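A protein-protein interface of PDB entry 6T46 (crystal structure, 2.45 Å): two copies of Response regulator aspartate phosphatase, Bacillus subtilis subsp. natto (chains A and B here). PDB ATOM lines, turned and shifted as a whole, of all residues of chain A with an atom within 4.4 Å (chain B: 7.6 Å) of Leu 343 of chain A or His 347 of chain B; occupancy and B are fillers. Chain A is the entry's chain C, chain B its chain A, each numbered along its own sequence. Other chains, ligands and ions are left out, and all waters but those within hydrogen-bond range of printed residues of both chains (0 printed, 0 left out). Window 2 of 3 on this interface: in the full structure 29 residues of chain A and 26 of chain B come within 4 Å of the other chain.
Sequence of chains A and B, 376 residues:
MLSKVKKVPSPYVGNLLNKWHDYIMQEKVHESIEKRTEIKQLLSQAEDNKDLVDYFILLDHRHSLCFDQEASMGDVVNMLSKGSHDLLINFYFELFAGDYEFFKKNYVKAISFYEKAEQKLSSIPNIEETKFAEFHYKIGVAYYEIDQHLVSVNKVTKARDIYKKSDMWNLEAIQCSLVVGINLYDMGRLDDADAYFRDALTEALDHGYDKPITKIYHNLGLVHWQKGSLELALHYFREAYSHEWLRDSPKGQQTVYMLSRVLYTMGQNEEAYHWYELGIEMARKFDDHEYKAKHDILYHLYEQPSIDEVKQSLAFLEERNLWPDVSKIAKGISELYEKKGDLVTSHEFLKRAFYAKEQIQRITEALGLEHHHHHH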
ATOM      1  N   GLU A 338       7.340 -25.873 -23.436  1.00  0.00           N
ATOM      2  CA  GLU A 338       8.522 -25.449 -24.167  1.00  0.00           C
ATOM      3  C   GLU A 338       8.145 -24.941 -25.551  1.00  0.00           C
ATOM      4  O   GLU A 338       8.622 -23.884 -25.975  1.00  0.00           O
ATOM      5  CB  GLU A 338       9.511 -26.597 -24.277  1.00  0.00           C
ATOM      6  CG  GLU A 338      10.753 -26.468 -23.431  1.00  0.00           C
ATOM      7  CD  GLU A 338      11.744 -27.584 -23.749  1.00  0.00           C
ATOM      8  OE1 GLU A 338      12.678 -27.806 -22.951  1.00  0.00           O
ATOM      9  OE2 GLU A 338      11.591 -28.250 -24.806  1.00  0.00           O
ATOM     10  N   GLY A 341       6.920 -21.536 -25.047  1.00  0.00           N
ATOM     11  CA  GLY A 341       7.985 -20.648 -24.629  1.00  0.00           C
ATOM     12  C   GLY A 341       7.958 -20.339 -23.148  1.00  0.00           C
ATOM     13  O   GLY A 341       8.721 -19.492 -22.664  1.00  0.00           O
ATOM     14  N   ASP A 342       7.130 -21.071 -22.403  1.00  0.00           N
ATOM     15  CA  ASP A 342       7.150 -20.958 -20.949  1.00  0.00           C
ATOM     16  C   ASP A 342       8.124 -22.026 -20.464  1.00  0.00           C
ATOM     17  O   ASP A 342       7.742 -23.186 -20.280  1.00  0.00           O
ATOM     18  CB  ASP A 342       5.753 -21.107 -20.353  1.00  0.00           C
ATOM     19  CG  ASP A 342       5.708 -20.698 -18.890  1.00  0.00           C
ATOM     20  OD1 ASP A 342       6.795 -20.532 -18.281  1.00  0.00           O
ATOM     21  OD2 ASP A 342       4.601 -20.497 -18.357  1.00  0.00           O
ATOM     22  N   LEU A 343       9.360 -21.615 -20.146  1.00  0.00           N
ATOM     23  CA  LEU A 343      10.331 -22.633 -19.802  1.00  0.00           C
ATOM     24  C   LEU A 343      10.355 -22.896 -18.315  1.00  0.00           C
ATOM     25  O   LEU A 343      10.628 -24.021 -17.907  1.00  0.00           O
ATOM     26  CB  LEU A 343      11.722 -22.222 -20.287  1.00  0.00           C
ATOM     27  CG  LEU A 343      12.935 -23.054 -19.832  1.00  0.00           C
ATOM     28  CD1 LEU A 343      12.680 -24.473 -20.269  1.00  0.00           C
ATOM     29  CD2 LEU A 343      14.279 -22.599 -20.387  1.00  0.00           C
ATOM     30  N   VAL A 344       9.951 -21.934 -17.492  1.00  0.00           N
ATOM     31  CA  VAL A 344       9.928 -22.177 -16.055  1.00  0.00           C
ATOM     32  C   VAL A 344       8.934 -23.301 -15.735  1.00  0.00           C
ATOM     33  O   VAL A 344       9.209 -24.188 -14.916  1.00  0.00           O
ATOM     34  CB  VAL A 344       9.637 -20.862 -15.293  1.00  0.00           C
ATOM     35  CG1 VAL A 344       8.233 -20.400 -15.527  1.00  0.00           C
ATOM     36  CG2 VAL A 344       9.901 -21.067 -13.824  1.00  0.00           C
ATOM     37  N   THR A 345       7.770 -23.297 -16.382  1.00  0.00           N
ATOM     38  CA  THR A 345       6.825 -24.377 -16.140  1.00  0.00           C
ATOM     39  C   THR A 345       7.155 -25.608 -16.970  1.00  0.00           C
ATOM     40  O   THR A 345       6.804 -26.721 -16.570  1.00  0.00           O
ATOM     41  CB  THR A 345       5.409 -23.891 -16.399  1.00  0.00           C
ATOM     42  OG1 THR A 345       5.232 -23.713 -17.809  1.00  0.00           O
ATOM     43  CG2 THR A 345       5.146 -22.583 -15.642  1.00  0.00           C
ATOM     44  N   SER A 346       7.804 -25.448 -18.127  1.00  0.00           N
ATOM     45  CA  SER A 346       8.268 -26.639 -18.829  1.00  0.00           C
ATOM     46  C   SER A 346       9.332 -27.356 -18.008  1.00  0.00           C
ATOM     47  O   SER A 346       9.348 -28.593 -17.927  1.00  0.00           O
ATOM     48  CB  SER A 346       8.844 -26.256 -20.192  1.00  0.00           C
ATOM     49  OG  SER A 346       9.869 -27.163 -20.575  1.00  0.00           O
ATOM     50  N   HIS A 347      10.204 -26.589 -17.348  1.00  0.00           N
ATOM     51  CA  HIS A 347      11.211 -27.192 -16.484  1.00  0.00           C
ATOM     52  C   HIS A 347      10.566 -27.787 -15.249  1.00  0.00           C
ATOM     53  O   HIS A 347      10.995 -28.846 -14.771  1.00  0.00           O
ATOM     54  CB  HIS A 347      12.266 -26.150 -16.128  1.00  0.00           C
ATOM     55  CG  HIS A 347      13.447 -26.685 -15.380  1.00  0.00           C
ATOM     56  ND1 HIS A 347      14.494 -27.330 -16.008  1.00  0.00           N
ATOM     57  CD2 HIS A 347      13.820 -26.537 -14.085  1.00  0.00           C
ATOM     58  CE1 HIS A 347      15.423 -27.629 -15.114  1.00  0.00           C
ATOM     59  NE2 HIS A 347      15.042 -27.154 -13.940  1.00  0.00           N
ATOM     60  N   LEU A 350       9.200 -31.100 -16.346  1.00  0.00           N
ATOM     61  CA  LEU A 350      10.299 -32.035 -16.579  1.00  0.00           C
ATOM     62  C   LEU A 350      10.855 -32.549 -15.253  1.00  0.00           C
ATOM     63  O   LEU A 350      11.067 -33.751 -15.087  1.00  0.00           O
ATOM     64  CB  LEU A 350      11.402 -31.362 -17.372  1.00  0.00           C
ATOM     65  CG  LEU A 350      12.417 -32.369 -17.844  1.00  0.00           C
ATOM     66  CD1 LEU A 350      11.707 -33.459 -18.603  1.00  0.00           C
ATOM     67  CD2 LEU A 350      13.395 -31.666 -18.723  1.00  0.00           C
ATOM     68  N   ILE B 333      24.412 -31.984 -12.459  1.00  0.00           N
ATOM     69  CA  ILE B 333      24.808 -30.789 -13.200  1.00  0.00           C
ATOM     70  C   ILE B 333      23.607 -29.889 -13.384  1.00  0.00           C
ATOM     71  O   ILE B 333      23.674 -28.679 -13.151  1.00  0.00           O
ATOM     72  CB  ILE B 333      25.430 -31.176 -14.548  1.00  0.00           C
ATOM     73  CG1 ILE B 333      26.765 -31.888 -14.318  1.00  0.00           C
ATOM     74  CG2 ILE B 333      25.558 -29.964 -15.407  1.00  0.00           C
ATOM     75  CD1 ILE B 333      27.170 -32.771 -15.435  1.00  0.00           C
ATOM     76  N   SER B 334      22.470 -30.488 -13.726  1.00  0.00           N
ATOM     77  CA  SER B 334      21.230 -29.740 -13.849  1.00  0.00           C
ATOM     78  C   SER B 334      20.923 -28.959 -12.586  1.00  0.00           C
ATOM     79  O   SER B 334      20.431 -27.834 -12.657  1.00  0.00           O
ATOM     80  CB  SER B 334      20.092 -30.709 -14.155  1.00  0.00           C
ATOM     81  OG  SER B 334      18.830 -30.102 -13.977  1.00  0.00           O
ATOM     82  N   GLU B 335      21.193 -29.540 -11.417  1.00  0.00           N
ATOM     83  CA  GLU B 335      20.896 -28.849 -10.165  1.00  0.00           C
ATOM     84  C   GLU B 335      21.873 -27.716  -9.897  1.00  0.00           C
ATOM     85  O   GLU B 335      21.469 -26.640  -9.424  1.00  0.00           O
ATOM     86  CB  GLU B 335      20.915 -29.856  -9.027  1.00  0.00           C
ATOM     87  CG  GLU B 335      19.625 -30.669  -8.956  1.00  0.00           C
ATOM     88  CD  GLU B 335      19.679 -31.786  -7.937  1.00  0.00           C
ATOM     89  OE1 GLU B 335      18.902 -32.752  -8.083  1.00  0.00           O
ATOM     90  OE2 GLU B 335      20.533 -31.720  -7.023  1.00  0.00           O
ATOM     91  N   TYR B 337      23.620 -25.853 -12.195  1.00  0.00           N
ATOM     92  CA  TYR B 337      23.391 -24.720 -13.072  1.00  0.00           C
ATOM     93  C   TYR B 337      22.122 -23.964 -12.722  1.00  0.00           C
ATOM     94  O   TYR B 337      22.052 -22.753 -12.940  1.00  0.00           O
ATOM     95  CB  TYR B 337      23.362 -25.194 -14.511  1.00  0.00           C
ATOM     96  CG  TYR B 337      24.752 -25.370 -15.033  1.00  0.00           C
ATOM     97  CD1 TYR B 337      25.833 -25.021 -14.253  1.00  0.00           C
ATOM     98  CD2 TYR B 337      24.993 -25.877 -16.303  1.00  0.00           C
ATOM     99  CE1 TYR B 337      27.112 -25.163 -14.712  1.00  0.00           C
ATOM    100  CE2 TYR B 337      26.276 -26.026 -16.772  1.00  0.00           C
ATOM    101  CZ  TYR B 337      27.325 -25.664 -15.968  1.00  0.00           C
ATOM    102  OH  TYR B 337      28.604 -25.802 -16.413  1.00  0.00           O
ATOM    103  N   GLU B 338      21.123 -24.631 -12.160  1.00  0.00           N
ATOM    104  CA  GLU B 338      19.944 -23.891 -11.734  1.00  0.00           C
ATOM    105  C   GLU B 338      20.252 -23.049 -10.507  1.00  0.00           C
ATOM    106  O   GLU B 338      19.809 -21.900 -10.407  1.00  0.00           O
ATOM    107  CB  GLU B 338      18.787 -24.834 -11.446  1.00  0.00           C
ATOM    108  CG  GLU B 338      17.625 -24.117 -10.789  1.00  0.00           C
ATOM    109  CD  GLU B 338      16.347 -24.933 -10.769  1.00  0.00           C
ATOM    110  OE1 GLU B 338      16.339 -26.089 -11.281  1.00  0.00           O
ATOM    111  OE2 GLU B 338      15.356 -24.407 -10.213  1.00  0.00           O
ATOM    112  N   ASP B 342      21.341 -20.168 -13.993  1.00  0.00           N
ATOM    113  CA  ASP B 342      21.267 -20.443 -15.422  1.00  0.00           C
ATOM    114  C   ASP B 342      20.192 -21.514 -15.617  1.00  0.00           C
ATOM    115  O   ASP B 342      20.406 -22.673 -15.245  1.00  0.00           O
ATOM    116  CB  ASP B 342      22.608 -20.939 -15.958  1.00  0.00           C
ATOM    117  CG  ASP B 342      22.682 -20.897 -17.486  1.00  0.00           C
ATOM    118  OD1 ASP B 342      21.671 -20.570 -18.153  1.00  0.00           O
ATOM    119  OD2 ASP B 342      23.744 -21.264 -18.030  1.00  0.00           O
ATOM    120  N   LEU B 343      19.061 -21.161 -16.250  1.00  0.00           N
ATOM    121  CA  LEU B 343      18.023 -22.170 -16.452  1.00  0.00           C
ATOM    122  C   LEU B 343      18.060 -22.825 -17.815  1.00  0.00           C
ATOM    123  O   LEU B 343      17.578 -23.958 -17.930  1.00  0.00           O
ATOM    124  CB  LEU B 343      16.614 -21.613 -16.259  1.00  0.00           C
ATOM    125  CG  LEU B 343      16.090 -21.450 -14.844  1.00  0.00           C
ATOM    126  CD1 LEU B 343      14.659 -20.962 -14.892  1.00  0.00           C
ATOM    127  CD2 LEU B 343      16.133 -22.805 -14.179  1.00  0.00           C
ATOM    128  N   VAL B 344      18.636 -22.194 -18.846  1.00  0.00           N
ATOM    129  CA  VAL B 344      18.659 -22.888 -20.135  1.00  0.00           C
ATOM    130  C   VAL B 344      19.514 -24.144 -20.053  1.00  0.00           C
ATOM    131  O   VAL B 344      19.078 -25.230 -20.467  1.00  0.00           O
ATOM    132  CB  VAL B 344      19.130 -21.974 -21.278  1.00  0.00           C
ATOM    133  CG1 VAL B 344      17.977 -21.122 -21.766  1.00  0.00           C
ATOM    134  CG2 VAL B 344      20.281 -21.097 -20.822  1.00  0.00           C
ATOM    135  N   THR B 345      20.696 -24.052 -19.424  1.00  0.00           N
ATOM    136  CA  THR B 345      21.547 -25.240 -19.377  1.00  0.00           C
ATOM    137  C   THR B 345      21.099 -26.210 -18.293  1.00  0.00           C
ATOM    138  O   THR B 345      21.160 -27.433 -18.496  1.00  0.00           O
ATOM    139  CB  THR B 345      23.021 -24.861 -19.179  1.00  0.00           C
ATOM    140  OG1 THR B 345      23.177 -24.186 -17.937  1.00  0.00           O
ATOM    141  CG2 THR B 345      23.503 -23.957 -20.295  1.00  0.00           C
ATOM    142  N   SER B 346      20.538 -25.705 -17.192  1.00  0.00           N
ATOM    143  CA  SER B 346      20.028 -26.623 -16.184  1.00  0.00           C
ATOM    144  C   SER B 346      18.896 -27.454 -16.752  1.00  0.00           C
ATOM    145  O   SER B 346      18.791 -28.650 -16.468  1.00  0.00           O
ATOM    146  CB  SER B 346      19.528 -25.857 -14.969  1.00  0.00           C
ATOM    147  OG  SER B 346      18.472 -26.599 -14.386  1.00  0.00           O
ATOM    148  N   HIS B 347      18.063 -26.838 -17.591  1.00  0.00           N
ATOM    149  CA  HIS B 347      16.998 -27.564 -18.268  1.00  0.00           C
ATOM    150  C   HIS B 347      17.562 -28.492 -19.342  1.00  0.00           C
ATOM    151  O   HIS B 347      16.989 -29.550 -19.620  1.00  0.00           O
ATOM    152  CB  HIS B 347      16.016 -26.557 -18.875  1.00  0.00           C
ATOM    153  CG  HIS B 347      14.760 -27.159 -19.418  1.00  0.00           C
ATOM    154  ND1 HIS B 347      13.646 -27.382 -18.641  1.00  0.00           N
ATOM    155  CD2 HIS B 347      14.434 -27.564 -20.665  1.00  0.00           C
ATOM    156  CE1 HIS B 347      12.681 -27.884 -19.390  1.00  0.00           C
ATOM    157  NE2 HIS B 347      13.137 -28.010 -20.621  1.00  0.00           N
ATOM    158  N   GLU B 348      18.659 -28.112 -19.988  1.00  0.00           N
ATOM    159  CA  GLU B 348      19.154 -29.011 -21.015  1.00  0.00           C
ATOM    160  C   GLU B 348      19.804 -30.240 -20.396  1.00  0.00           C
ATOM    161  O   GLU B 348      19.736 -31.327 -20.972  1.00  0.00           O
ATOM    162  CB  GLU B 348      20.076 -28.272 -21.978  1.00  0.00           C
ATOM    163  CG  GLU B 348      21.545 -28.307 -21.689  1.00  0.00           C
ATOM    164  CD  GLU B 348      22.336 -28.109 -22.983  1.00  0.00           C
ATOM    165  OE1 GLU B 348      23.518 -27.680 -22.937  1.00  0.00           O
ATOM    166  OE2 GLU B 348      21.751 -28.395 -24.059  1.00  0.00           O
ATOM    167  N   PHE B 349      20.404 -30.104 -19.210  1.00  0.00           N
ATOM    168  CA  PHE B 349      20.973 -31.279 -18.559  1.00  0.00           C
ATOM    169  C   PHE B 349      19.869 -32.129 -17.943  1.00  0.00           C
ATOM    170  O   PHE B 349      19.971 -33.364 -17.925  1.00  0.00           O
ATOM    171  CB  PHE B 349      22.000 -30.864 -17.497  1.00  0.00           C
ATOM    172  CG  PHE B 349      23.391 -30.630 -18.055  1.00  0.00           C
ATOM    173  CD1 PHE B 349      24.256 -31.680 -18.266  1.00  0.00           C
ATOM    174  CD2 PHE B 349      23.815 -29.349 -18.395  1.00  0.00           C
ATOM    175  CE1 PHE B 349      25.530 -31.466 -18.800  1.00  0.00           C
ATOM    176  CE2 PHE B 349      25.074 -29.132 -18.924  1.00  0.00           C
ATOM    177  CZ  PHE B 349      25.930 -30.195 -19.132  1.00  0.00           C
ATOM    178  N   LEU B 350      18.804 -31.492 -17.454  1.00  0.00           N
ATOM    179  CA  LEU B 350      17.651 -32.255 -16.992  1.00  0.00           C
ATOM    180  C   LEU B 350      17.051 -33.081 -18.114  1.00  0.00           C
ATOM    181  O   LEU B 350      16.661 -34.234 -17.897  1.00  0.00           O
ATOM    182  CB  LEU B 350      16.604 -31.318 -16.425  1.00  0.00           C
ATOM    183  CG  LEU B 350      15.488 -32.093 -15.782  1.00  0.00           C
ATOM    184  CD1 LEU B 350      16.095 -33.119 -14.850  1.00  0.00           C
ATOM    185  CD2 LEU B 350      14.673 -31.079 -15.000  1.00  0.00           C
ATOM    186  N   LYS B 351      16.960 -32.509 -19.322  1.00  0.00           N
ATOM    187  CA  LYS B 351      16.548 -33.293 -20.486  1.00  0.00           C
ATOM    188  C   LYS B 351      17.494 -34.471 -20.717  1.00  0.00           C
ATOM    189  O   LYS B 351      17.057 -35.580 -21.054  1.00  0.00           O
ATOM    190  CB  LYS B 351      16.460 -32.385 -21.709  1.00  0.00           C
ATOM    191  CG  LYS B 351      15.138 -31.643 -21.705  1.00  0.00           C
ATOM    192  CD  LYS B 351      14.786 -30.954 -22.999  1.00  0.00           C
ATOM    193  CE  LYS B 351      15.417 -29.594 -23.085  1.00  0.00           C
ATOM    194  NZ  LYS B 351      14.667 -28.745 -24.067  1.00  0.00           N
ATOM    195  N   ARG B 352      18.790 -34.265 -20.516  1.00  0.00           N
ATOM    196  CA  ARG B 352      19.715 -35.367 -20.735  1.00  0.00           C
ATOM    197  C   ARG B 352      19.628 -36.404 -19.616  1.00  0.00           C
ATOM    198  O   ARG B 352      19.829 -37.602 -19.857  1.00  0.00           O
ATOM    199  CB  ARG B 352      21.127 -34.809 -20.845  1.00  0.00           C
ATOM    200  CG  ARG B 352      21.358 -34.244 -22.218  1.00  0.00           C
ATOM    201  CD  ARG B 352      22.770 -33.771 -22.446  1.00  0.00           C
ATOM    202  NE  ARG B 352      23.676 -34.900 -22.566  1.00  0.00           N
ATOM    203  CZ  ARG B 352      24.840 -34.817 -23.184  1.00  0.00           C
ATOM    204  NH1 ARG B 352      25.623 -35.888 -23.265  1.00  0.00           N
ATOM    205  NH2 ARG B 352      25.193 -33.661 -23.746  1.00  0.00           N
ATOM    206  N   ALA B 353      19.360 -35.965 -18.385  1.00  0.00           N
ATOM    207  CA  ALA B 353      19.156 -36.912 -17.294  1.00  0.00           C
ATOM    208  C   ALA B 353      17.905 -37.731 -17.511  1.00  0.00           C
ATOM    209  O   ALA B 353      17.874 -38.918 -17.184  1.00  0.00           O
ATOM    210  CB  ALA B 353      19.055 -36.185 -15.959  1.00  0.00           C
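Leu 343 of chain A touches just one residue of chain B: His 347 (3.5 Å).
His 347 of chain B touches five residues of chain A.
Of the printed residues of chain A, Glu 338 of chain B touches His 347.
Of the printed residues of chain B, Ser 346 of chain A touches His 347.
Of the printed residues of chain A, Lys 351 of chain B touches Glu 338 and Leu 350.
Of the printed residues of chain A, Leu 350 of chain B touches His 347 and Leu 350.
Asp 342 of chain B touches none of the printed residues of chain A.
Leu 343 of chain B touches none of the printed residues of chain A.
The nearest printed residue of chain A that does not touch Ser 346 of chain B is Leu 350 of chain A (6.6 Å).
O of Ser 346 of chain B is in hydrogen-bond range of OG of Ser 334 of chain B (2.9 Å).
Of the 9 printed residues of chain A, 5 touch a printed residue of chain B.
Among the printed residues, Asp or Glu carboxylates within 4 Å of a Lys or Arg side-chain nitrogen of the other chain: Glu 338 of chain A with Lys 351 of chain B (2.5 Å).
Among the printed residues, pairs that only touch across the chains: His 347 of chain A with Ser 346 of chain B (3.3 Å), Leu 350 of chain A with Lys 351 of chain B (3.5 Å), Leu 343 of chain A with His 347 of chain B (3.5 Å), His 347 of chain A with Leu 350 of chain B (3.5 Å), Leu 350 of chain A with Leu 350 of chain B (3.6 Å) and Leu 350 of chain A with His 347 of chain B (3.9 Å).
The side-chain carboxylate (OE1) of Glu 338 of chain B lies within hydrogen-bond range of a ring nitrogen (NE2) of His 347 of chain A (3.1 Å).
A ring nitrogen (NE2) of His 347 of chain B sits close to the side-chain hydroxyl of Ser 346 of chain A.
A ring nitrogen (ND1) of His 347 of chain B lies within hydrogen-bond range of a ring nitrogen (ND1) of His 347 of chain A, at 2.8 Å.
The side-chain amino group (NZ) of Lys 351 of chain B lies within salt-bridge range of the side-chain carboxylate (OE1) of Glu 338 of chain A.
A ring nitrogen (NE2) of His 347 of chain B sits close to the side-chain carboxylate of Glu 338 of chain A (2.4 Å).
Glu 338 of chain A touches His 347 of chain B, and with the chains exchanged His 347 of chain A touches Glu 338 of chain B.
Leu 343 of chain A touches His 347 of chain B, but with the chains exchanged His 347 of chain A does not touch Leu 343 of chain B (4.4 Å).
His 347 of chain A touches Leu 350 of chain B, and with the chains exchanged Leu 350 of chain A touches His 347 of chain B.
Leu 350 of chain A touches its own counterpart, Leu 350 of chain B.
Positions printed for both chains: 338, 342, 343, 344, 345, 346, 347 and 350.
Of the 11 pairs that touch across the chains among the printed residues, 8 have their exchanged pair printed and touching as well.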
